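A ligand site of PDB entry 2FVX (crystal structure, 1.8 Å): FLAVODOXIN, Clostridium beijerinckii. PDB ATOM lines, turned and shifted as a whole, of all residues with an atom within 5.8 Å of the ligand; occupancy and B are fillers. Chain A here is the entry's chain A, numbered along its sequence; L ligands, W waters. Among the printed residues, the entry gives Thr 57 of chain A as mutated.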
ATOM      1  N   TRP A   6       7.099  14.289  15.612  1.00  0.00           N
ATOM      2  CA  TRP A   6       8.545  14.288  15.385  1.00  0.00           C
ATOM      3  C   TRP A   6       8.995  15.589  16.077  1.00  0.00           C
ATOM      4  O   TRP A   6       8.331  16.619  15.965  1.00  0.00           O
ATOM      5  CB  TRP A   6       8.928  14.352  13.893  1.00  0.00           C
ATOM      6  CG  TRP A   6      10.416  14.285  13.725  1.00  0.00           C
ATOM      7  CD1 TRP A   6      11.183  13.149  13.669  1.00  0.00           C
ATOM      8  CD2 TRP A   6      11.348  15.387  13.720  1.00  0.00           C
ATOM      9  NE1 TRP A   6      12.522  13.480  13.657  1.00  0.00           N
ATOM     10  CE2 TRP A   6      12.648  14.847  13.686  1.00  0.00           C
ATOM     11  CE3 TRP A   6      11.198  16.787  13.749  1.00  0.00           C
ATOM     12  CZ2 TRP A   6      13.804  15.656  13.690  1.00  0.00           C
ATOM     13  CZ3 TRP A   6      12.346  17.589  13.740  1.00  0.00           C
ATOM     14  CH2 TRP A   6      13.633  17.010  13.713  1.00  0.00           C
ATOM     15  N   SER A   7      10.105  15.521  16.802  1.00  0.00           N
ATOM     16  CA  SER A   7      10.635  16.704  17.483  1.00  0.00           C
ATOM     17  C   SER A   7      12.162  16.623  17.458  1.00  0.00           C
ATOM     18  O   SER A   7      12.753  15.592  17.805  1.00  0.00           O
ATOM     19  CB  SER A   7      10.128  16.767  18.924  1.00  0.00           C
ATOM     20  OG  SER A   7      10.568  17.943  19.574  1.00  0.00           O
ATOM     21  N   GLY A   8      12.795  17.723  17.041  1.00  0.00           N
ATOM     22  CA  GLY A   8      14.256  17.757  16.951  1.00  0.00           C
ATOM     23  C   GLY A   8      14.959  18.193  18.217  1.00  0.00           C
ATOM     24  O   GLY A   8      16.054  17.734  18.497  1.00  0.00           O
ATOM     25  N   THR A   9      14.352  19.117  18.964  1.00  0.00           N
ATOM     26  CA  THR A   9      14.973  19.586  20.199  1.00  0.00           C
ATOM     27  C   THR A   9      14.054  19.412  21.420  1.00  0.00           C
ATOM     28  O   THR A   9      14.459  19.711  22.548  1.00  0.00           O
ATOM     29  CB  THR A   9      15.409  21.076  20.094  1.00  0.00           C
ATOM     30  OG1 THR A   9      14.264  21.929  20.070  1.00  0.00           O
ATOM     31  CG2 THR A   9      16.211  21.316  18.824  1.00  0.00           C
ATOM     32  N   GLY A  10      12.824  18.956  21.203  1.00  0.00           N
ATOM     33  CA  GLY A  10      11.915  18.735  22.317  1.00  0.00           C
ATOM     34  C   GLY A  10      10.745  19.690  22.408  1.00  0.00           C
ATOM     35  O   GLY A  10       9.873  19.499  23.247  1.00  0.00           O
ATOM     36  N   ASN A  11      10.669  20.688  21.535  1.00  0.00           N
ATOM     37  CA  ASN A  11       9.571  21.646  21.603  1.00  0.00           C
ATOM     38  C   ASN A  11       8.227  21.027  21.233  1.00  0.00           C
ATOM     39  O   ASN A  11       7.254  21.156  21.985  1.00  0.00           O
ATOM     40  CB  ASN A  11       9.885  22.906  20.775  1.00  0.00           C
ATOM     41  CG  ASN A  11      11.041  23.685  21.380  1.00  0.00           C
ATOM     42  OD1 ASN A  11      11.334  23.531  22.567  1.00  0.00           O
ATOM     43  ND2 ASN A  11      11.738  24.466  20.556  1.00  0.00           N
ATOM     44  N   THR A  12       8.177  20.335  20.099  1.00  0.00           N
ATOM     45  CA  THR A  12       6.952  19.665  19.655  1.00  0.00           C
ATOM     46  C   THR A  12       6.611  18.485  20.582  1.00  0.00           C
ATOM     47  O   THR A  12       5.438  18.188  20.820  1.00  0.00           O
ATOM     48  CB  THR A  12       7.081  19.195  18.191  1.00  0.00           C
ATOM     49  OG1 THR A  12       7.348  20.355  17.374  1.00  0.00           O
ATOM     50  CG2 THR A  12       5.787  18.573  17.693  1.00  0.00           C
ATOM     51  N   GLU A  13       7.640  17.850  21.140  1.00  0.00           N
ATOM     52  CA  GLU A  13       7.437  16.753  22.085  1.00  0.00           C
ATOM     53  C   GLU A  13       6.698  17.264  23.327  1.00  0.00           C
ATOM     54  O   GLU A  13       5.770  16.630  23.813  1.00  0.00           O
ATOM     55  CB  GLU A  13       8.788  16.153  22.500  1.00  0.00           C
ATOM     56  CG  GLU A  13       8.626  14.962  23.429  1.00  0.00           C
ATOM     57  CD  GLU A  13       9.944  14.323  23.842  1.00  0.00           C
ATOM     58  OE1 GLU A  13      10.939  15.055  24.051  1.00  0.00           O
ATOM     59  OE2 GLU A  13       9.982  13.091  23.966  1.00  0.00           O
ATOM     60  N   SER A  54       7.615  19.929  13.862  1.00  0.00           N
ATOM     61  CA  SER A  54       8.093  21.304  13.797  1.00  0.00           C
ATOM     62  C   SER A  54       8.438  21.707  12.351  1.00  0.00           C
ATOM     63  O   SER A  54       8.535  20.840  11.463  1.00  0.00           O
ATOM     64  CB  SER A  54       9.335  21.447  14.666  1.00  0.00           C
ATOM     65  OG  SER A  54      10.256  20.414  14.357  1.00  0.00           O
ATOM     66  N   ALA A  55       8.611  23.007  12.133  1.00  0.00           N
ATOM     67  CA  ALA A  55       8.963  23.518  10.816  1.00  0.00           C
ATOM     68  C   ALA A  55      10.437  23.199  10.590  1.00  0.00           C
ATOM     69  O   ALA A  55      11.280  23.436  11.469  1.00  0.00           O
ATOM     70  CB  ALA A  55       8.721  25.012  10.763  1.00  0.00           C
ATOM     71  N   MET A  56      10.758  22.626   9.439  1.00  0.00           N
ATOM     72  CA  MET A  56      12.146  22.273   9.158  1.00  0.00           C
ATOM     73  C   MET A  56      12.621  22.744   7.789  1.00  0.00           C
ATOM     74  O   MET A  56      11.815  23.136   6.938  1.00  0.00           O
ATOM     75  CB  MET A  56      12.352  20.771   9.314  1.00  0.00           C
ATOM     76  CG  MET A  56      12.130  20.272  10.739  1.00  0.00           C
ATOM     77  SD  MET A  56      13.219  21.084  11.972  1.00  0.00           S
ATOM     78  CE  MET A  56      14.703  20.210  11.670  1.00  0.00           C
ATOM     79  N   THR A  57      13.935  22.742   7.615  1.00  0.00           N
ATOM     80  CA  THR A  57      14.571  23.185   6.374  1.00  0.00           C
ATOM     81  C   THR A  57      14.077  24.603   6.090  1.00  0.00           C
ATOM     82  O   THR A  57      14.521  25.555   6.716  1.00  0.00           O
ATOM     83  CB  THR A  57      14.242  22.201   5.204  1.00  0.00           C
ATOM     84  OG1 THR A  57      14.567  20.854   5.612  1.00  0.00           O
ATOM     85  CG2 THR A  57      15.041  22.548   3.964  1.00  0.00           C
ATOM     86  N   ASP A  58      13.126  24.728   5.166  1.00  0.00           N
ATOM     87  CA  ASP A  58      12.536  26.027   4.851  1.00  0.00           C
ATOM     88  C   ASP A  58      11.044  25.808   4.673  1.00  0.00           C
ATOM     89  O   ASP A  58      10.574  25.468   3.586  1.00  0.00           O
ATOM     90  CB  ASP A  58      13.145  26.634   3.585  1.00  0.00           C
ATOM     91  CG  ASP A  58      12.504  27.971   3.219  1.00  0.00           C
ATOM     92  OD1 ASP A  58      12.191  28.768   4.115  1.00  0.00           O
ATOM     93  OD2 ASP A  58      12.299  28.211   2.010  1.00  0.00           O
ATOM     94  N   GLU A  59      10.318  25.920   5.783  1.00  0.00           N
ATOM     95  CA  GLU A  59       8.873  25.780   5.825  1.00  0.00           C
ATOM     96  C   GLU A  59       8.309  24.475   5.289  1.00  0.00           C
ATOM     97  O   GLU A  59       7.310  24.490   4.558  1.00  0.00           O
ATOM     98  CB  GLU A  59       8.180  26.964   5.133  1.00  0.00           C
ATOM     99  CG  GLU A  59       8.498  28.334   5.708  1.00  0.00           C
ATOM    100  CD  GLU A  59       8.077  28.522   7.161  1.00  0.00           C
ATOM    101  OE1 GLU A  59       7.035  27.975   7.592  1.00  0.00           O
ATOM    102  OE2 GLU A  59       8.795  29.239   7.883  1.00  0.00           O
ATOM    103  N   VAL A  60       8.928  23.347   5.638  1.00  0.00           N
ATOM    104  CA  VAL A  60       8.422  22.038   5.205  1.00  0.00           C
ATOM    105  C   VAL A  60       8.416  21.086   6.398  1.00  0.00           C
ATOM    106  O   VAL A  60       8.875  21.444   7.496  1.00  0.00           O
ATOM    107  CB  VAL A  60       9.251  21.411   4.051  1.00  0.00           C
ATOM    108  CG1 VAL A  60       9.123  22.252   2.793  1.00  0.00           C
ATOM    109  CG2 VAL A  60      10.717  21.254   4.471  1.00  0.00           C
ATOM    110  N   SER A  87       5.698  23.148  16.611  1.00  0.00           N
ATOM    111  CA  SER A  87       6.442  24.329  17.025  1.00  0.00           C
ATOM    112  C   SER A  87       7.203  24.852  15.820  1.00  0.00           C
ATOM    113  O   SER A  87       7.504  24.106  14.886  1.00  0.00           O
ATOM    114  CB  SER A  87       7.410  23.941  18.159  1.00  0.00           C
ATOM    115  OG  SER A  87       8.156  25.055  18.633  1.00  0.00           O
ATOM    116  N   TYR A  88       7.497  26.154  15.828  1.00  0.00           N
ATOM    117  CA  TYR A  88       8.235  26.767  14.743  1.00  0.00           C
ATOM    118  C   TYR A  88       9.172  27.811  15.329  1.00  0.00           C
ATOM    119  O   TYR A  88       9.054  28.164  16.499  1.00  0.00           O
ATOM    120  CB  TYR A  88       7.321  27.373  13.699  1.00  0.00           C
ATOM    121  CG  TYR A  88       6.495  28.515  14.219  1.00  0.00           C
ATOM    122  CD1 TYR A  88       5.353  28.278  14.971  1.00  0.00           C
ATOM    123  CD2 TYR A  88       6.849  29.821  13.938  1.00  0.00           C
ATOM    124  CE1 TYR A  88       4.575  29.318  15.422  1.00  0.00           C
ATOM    125  CE2 TYR A  88       6.081  30.878  14.388  1.00  0.00           C
ATOM    126  CZ  TYR A  88       4.937  30.618  15.124  1.00  0.00           C
ATOM    127  OH  TYR A  88       4.145  31.652  15.535  1.00  0.00           O
ATOM    128  N   GLY A  89      10.099  28.320  14.522  1.00  0.00           N
ATOM    129  CA  GLY A  89      11.065  29.252  15.057  1.00  0.00           C
ATOM    130  C   GLY A  89      11.003  30.686  14.610  1.00  0.00           C
ATOM    131  O   GLY A  89      10.924  31.574  15.452  1.00  0.00           O
ATOM    132  N   TRP A  90      11.055  30.932  13.307  1.00  0.00           N
ATOM    133  CA  TRP A  90      11.081  32.311  12.808  1.00  0.00           C
ATOM    134  C   TRP A  90      10.035  32.682  11.769  1.00  0.00           C
ATOM    135  O   TRP A  90       9.832  33.861  11.497  1.00  0.00           O
ATOM    136  CB  TRP A  90      12.474  32.635  12.259  1.00  0.00           C
ATOM    137  CG  TRP A  90      12.975  31.628  11.241  1.00  0.00           C
ATOM    138  CD1 TRP A  90      12.665  31.574   9.919  1.00  0.00           C
ATOM    139  CD2 TRP A  90      13.861  30.524  11.494  1.00  0.00           C
ATOM    140  NE1 TRP A  90      13.289  30.511   9.327  1.00  0.00           N
ATOM    141  CE2 TRP A  90      14.032  29.847  10.268  1.00  0.00           C
ATOM    142  CE3 TRP A  90      14.528  30.044  12.625  1.00  0.00           C
ATOM    143  CZ2 TRP A  90      14.832  28.712  10.147  1.00  0.00           C
ATOM    144  CZ3 TRP A  90      15.323  28.900  12.505  1.00  0.00           C
ATOM    145  CH2 TRP A  90      15.468  28.250  11.279  1.00  0.00           C
ATOM    146  N   GLY A  91       9.406  31.699  11.154  1.00  0.00           N
ATOM    147  CA  GLY A  91       8.404  31.988  10.144  1.00  0.00           C
ATOM    148  C   GLY A  91       7.083  32.382  10.776  1.00  0.00           C
ATOM    149  O   GLY A  91       7.031  32.742  11.954  1.00  0.00           O
ATOM    150  N   ASP A  92       6.013  32.319   9.990  1.00  0.00           N
ATOM    151  CA  ASP A  92       4.681  32.641  10.488  1.00  0.00           C
ATOM    152  C   ASP A  92       3.680  31.517  10.253  1.00  0.00           C
ATOM    153  O   ASP A  92       2.485  31.752  10.097  1.00  0.00           O
ATOM    154  CB  ASP A  92       4.177  33.977   9.910  1.00  0.00           C
ATOM    155  CG  ASP A  92       4.106  33.991   8.379  1.00  0.00           C
ATOM    156  OD1 ASP A  92       3.926  32.919   7.743  1.00  0.00           O
ATOM    157  OD2 ASP A  92       4.219  35.106   7.820  1.00  0.00           O
ATOM    158  N   TRP A  95       4.663  26.333   6.876  1.00  0.00           N
ATOM    159  CA  TRP A  95       4.737  24.874   6.854  1.00  0.00           C
ATOM    160  C   TRP A  95       3.430  24.230   7.338  1.00  0.00           C
ATOM    161  O   TRP A  95       3.004  23.192   6.811  1.00  0.00           O
ATOM    162  CB  TRP A  95       5.945  24.371   7.657  1.00  0.00           C
ATOM    163  CG  TRP A  95       5.651  23.770   9.012  1.00  0.00           C
ATOM    164  CD1 TRP A  95       5.698  22.443   9.353  1.00  0.00           C
ATOM    165  CD2 TRP A  95       5.280  24.468  10.198  1.00  0.00           C
ATOM    166  NE1 TRP A  95       5.394  22.287  10.683  1.00  0.00           N
ATOM    167  CE2 TRP A  95       5.128  23.520  11.221  1.00  0.00           C
ATOM    168  CE3 TRP A  95       5.058  25.823  10.501  1.00  0.00           C
ATOM    169  CZ2 TRP A  95       4.770  23.871  12.540  1.00  0.00           C
ATOM    170  CZ3 TRP A  95       4.702  26.184  11.806  1.00  0.00           C
ATOM    171  CH2 TRP A  95       4.556  25.197  12.810  1.00  0.00           C
ATOM    172  N   VAL A 117       2.973  26.892  18.009  1.00  0.00           N
ATOM    173  CA  VAL A 117       3.570  27.668  19.097  1.00  0.00           C
ATOM    174  C   VAL A 117       4.999  27.945  18.691  1.00  0.00           C
ATOM    175  O   VAL A 117       5.650  27.076  18.112  1.00  0.00           O
ATOM    176  CB  VAL A 117       3.575  26.833  20.419  1.00  0.00           C
ATOM    177  CG1 VAL A 117       4.351  27.540  21.506  1.00  0.00           C
ATOM    178  CG2 VAL A 117       2.130  26.581  20.868  1.00  0.00           C
ATOM    179  N   GLN A 118       5.468  29.160  18.951  1.00  0.00           N
ATOM    180  CA  GLN A 118       6.824  29.518  18.595  1.00  0.00           C
ATOM    181  C   GLN A 118       7.761  29.052  19.695  1.00  0.00           C
ATOM    182  O   GLN A 118       7.548  29.356  20.869  1.00  0.00           O
ATOM    183  CB  GLN A 118       6.929  31.035  18.429  1.00  0.00           C
ATOM    184  CG  GLN A 118       8.240  31.521  17.874  1.00  0.00           C
ATOM    185  CD  GLN A 118       8.244  33.011  17.641  1.00  0.00           C
ATOM    186  OE1 GLN A 118       7.557  33.770  18.336  1.00  0.00           O
ATOM    187  NE2 GLN A 118       9.007  33.454  16.656  1.00  0.00           N
ATOM    188  N   ASN A 119       8.795  28.308  19.315  1.00  0.00           N
ATOM    189  CA  ASN A 119       9.791  27.775  20.244  1.00  0.00           C
ATOM    190  C   ASN A 119       9.120  26.889  21.309  1.00  0.00           C
ATOM    191  O   ASN A 119       8.079  26.274  21.045  1.00  0.00           O
ATOM    192  CB  ASN A 119      10.597  28.911  20.895  1.00  0.00           C
ATOM    193  CG  ASN A 119      11.106  29.928  19.854  1.00  0.00           C
ATOM    194  OD1 ASN A 119      11.954  29.600  19.014  1.00  0.00           O
ATOM    195  ND2 ASN A 119      10.553  31.134  19.888  1.00  0.00           N
ATOM    196  N   GLU A 120       9.675  26.839  22.510  1.00  0.00           N
ATOM    197  CA  GLU A 120       9.117  25.991  23.559  1.00  0.00           C
ATOM    198  C   GLU A 120       7.782  26.514  24.101  1.00  0.00           C
ATOM    199  O   GLU A 120       7.583  27.727  24.208  1.00  0.00           O
ATOM    200  CB  GLU A 120      10.137  25.873  24.693  1.00  0.00           C
ATOM    201  CG  GLU A 120       9.833  24.792  25.698  1.00  0.00           C
ATOM    202  CD  GLU A 120      10.734  24.855  26.929  1.00  0.00           C
ATOM    203  OE1 GLU A 120      11.415  25.885  27.129  1.00  0.00           O
ATOM    204  OE2 GLU A 120      10.751  23.862  27.700  1.00  0.00           O
HETATM  205  N1  LIG L   1      11.322  27.504  12.008  1.00  0.00           N
HETATM  206  C1  LIG L   1      10.494  28.239  11.222  1.00  0.00           C
HETATM  207  O1  LIG L   1       9.695  29.037  11.691  1.00  0.00           O
HETATM  208  N2  LIG L   1      10.582  28.074   9.803  1.00  0.00           N
HETATM  209  C2  LIG L   1      11.496  27.267   9.148  1.00  0.00           C
HETATM  210  O2  LIG L   1      11.545  27.218   7.927  1.00  0.00           O
HETATM  211  C3  LIG L   1      12.400  26.494  10.023  1.00  0.00           C
HETATM  212  N3  LIG L   1      13.365  25.746   9.491  1.00  0.00           N
HETATM  213  C4  LIG L   1      14.264  25.161  10.366  1.00  0.00           C
HETATM  214  C5  LIG L   1      15.385  24.440   9.880  1.00  0.00           C
HETATM  215  C6  LIG L   1      16.255  23.776  10.698  1.00  0.00           C
HETATM  216  C7  LIG L   1      17.437  23.026  10.124  1.00  0.00           C
HETATM  217  C8  LIG L   1      16.050  23.823  12.100  1.00  0.00           C
HETATM  218  C9  LIG L   1      16.895  23.054  13.062  1.00  0.00           C
HETATM  219  C10 LIG L   1      15.013  24.588  12.613  1.00  0.00           C
HETATM  220  C11 LIG L   1      14.093  25.222  11.768  1.00  0.00           C
HETATM  221  N4  LIG L   1      13.061  26.018  12.260  1.00  0.00           N
HETATM  222  C12 LIG L   1      12.190  26.685  11.464  1.00  0.00           C
HETATM  223  C13 LIG L   1      12.935  26.197  13.725  1.00  0.00           C
HETATM  224  C14 LIG L   1      12.184  25.082  14.466  1.00  0.00           C
HETATM  225  O3  LIG L   1      10.929  24.813  13.860  1.00  0.00           O
HETATM  226  C15 LIG L   1      11.961  25.513  15.919  1.00  0.00           C
HETATM  227  O4  LIG L   1      13.228  25.651  16.579  1.00  0.00           O
HETATM  228  C16 LIG L   1      11.053  24.553  16.735  1.00  0.00           C
HETATM  229  O5  LIG L   1      10.810  25.091  18.034  1.00  0.00           O
HETATM  230  C17 LIG L   1      11.712  23.182  16.899  1.00  0.00           C
HETATM  231  O6  LIG L   1      10.829  22.298  17.511  1.00  0.00           O
HETATM  232  P1  LIG L   1      11.313  20.832  17.867  1.00  0.00           P
HETATM  233  O7  LIG L   1      10.041  20.129  18.107  1.00  0.00           O
HETATM  234  O8  LIG L   1      12.277  20.861  18.965  1.00  0.00           O
HETATM  235  O9  LIG L   1      11.993  20.286  16.607  1.00  0.00           O
HETATM  236  O   HOH W   1      14.317  21.047  15.456  1.00  0.00           O
HETATM  237  O   HOH W   2      15.004  23.506  16.298  1.00  0.00           O
HETATM  238  O   HOH W   3       6.699  28.934  10.285  1.00  0.00           O
HETATM  239  O   HOH W   4      13.264  27.030  18.896  1.00  0.00           O
HETATM  240  O   HOH W   5      12.632  29.375   6.767  1.00  0.00           O
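The backbone NH (N) of Thr 9 sits at hydrogen-bond distance from an oxygen (O8) of the ligand (2.7 Å). An oxygen (O8) of the ligand is in hydrogen-bond range of the side-chain hydroxyl (OG1) of Thr 9, 2.5 Å away. The side-chain hydroxyl of Ser 7 lies within hydrogen-bond range of an oxygen (O7) of the ligand (2.7 Å). N of Gly 8 is in hydrogen-bond range of O9 of the ligand (2.7 Å). The side-chain hydroxyl (OG) of Ser 87 sits at hydrogen-bond distance from an oxygen (O5) of the ligand (2.7 Å). N of Gly 91 is in hydrogen-bond range of O1 of the ligand (2.7 Å). The backbone NH of Thr 12 lies within hydrogen-bond range of an oxygen (O7) of the ligand (2.7 Å). OG1 of Thr 12 is in hydrogen-bond range of O7 of the ligand. O8 of the ligand is in hydrogen-bond range of N of Asn 11 (3.0 Å). O5 of the ligand is in hydrogen-bond range of ND2 of Asn 11, at 2.8 Å. The backbone NH (N) of Ala 55 lies within hydrogen-bond range of an oxygen (O3) of the ligand, 3.4 Å away. The backbone carbonyl oxygen (O) of Ala 55 lies within hydrogen-bond range of an oxygen (O3) of the ligand, 2.8 Å away. The backbone NH (N) of Glu 59 sits at hydrogen-bond distance from an oxygen (O2) of the ligand. OE2 of Glu 59 sits at hydrogen-bond distance from N2 of the ligand (2.9 Å). An oxygen (O1) of the ligand is in hydrogen-bond range of the backbone NH (N) of Trp 90, 2.8 Å away. The side-chain hydroxyl of Ser 54 lies within hydrogen-bond range of an oxygen (O9) of the ligand, 2.8 Å away. The backbone NH (N) of Gly 89 lies within hydrogen-bond range of a nitrogen (N1) of the ligand. The backbone NH (N) of Gly 10 sits at hydrogen-bond distance from an oxygen (O8) of the ligand (3.0 Å).
The backbone NH (N) of Gly 10 sits at hydrogen-bond distance from the side-chain hydroxyl (OG) of Ser 7, at 3.0 Å. N of Glu 13 is in hydrogen-bond range of OG of Ser 7 (3.3 Å). The backbone NH of Ala 55 sits at hydrogen-bond distance from the backbone carbonyl oxygen of Ser 87 (3.2 Å). OG of Ser 87 lies within hydrogen-bond range of O of Asn 119 (2.7 Å). O of Val 117 lies close to OG of Ser 87 (3.3 Å). OE1 of Glu 59 sits at hydrogen-bond distance from N of Trp 95, at 3.0 Å. NE2 of Gln 118 sits at hydrogen-bond distance from O of Gly 89 (2.9 Å). N of Tyr 88 lies within hydrogen-bond range of O of Val 117 (3.1 Å).
A nitrogen (N3) of the ligand lies close to the backbone carbonyl oxygen (O) of Thr 57 (3.0 Å). Residues that only touch the ligand: Tyr 88 (3.4 Å), Asp 58 (3.4 Å), Met 56 (3.5 Å), Asn 119 (3.6 Å) and Trp 6 (3.95 Å). Hydrophobic or aromatic side chains that line the ligand: Trp 6, Ala 55, Met 56, Tyr 88 and Trp 90. 19 residues have an atom within 4 Å of the ligand: Trp 6, Ser 7, Gly 8, Thr 9, Gly 10, Asn 11, Thr 12, Ser 54, Ala 55, Met 56, Thr 57, Asp 58, Glu 59, Ser 87, Tyr 88, Gly 89, Trp 90, Gly 91 and Asn 119.
Water W5 lies within hydrogen-bond range of an oxygen (O2) of the ligand (2.7 Å), the side-chain carboxylate of Asp 58 (2.8 Å) and the indole nitrogen of Trp 90 (2.9 Å). Water W4 lies within hydrogen-bond range of an oxygen (O4) of the ligand (2.7 Å), the side-chain amide oxygen of Asn 119 (2.9 Å) and the side-chain amide nitrogen of Asn 11 (3.4 Å). Water W1 lies within hydrogen-bond range of an oxygen (O9) of the ligand and the side-chain sulfur of Met 56. Water W3 lies within hydrogen-bond range of the side-chain carboxylate of Glu 59 (2.9 Å), an oxygen (O1) of the ligand (3.3 Å) and the backbone NH of Asp 92 (3.5 Å).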
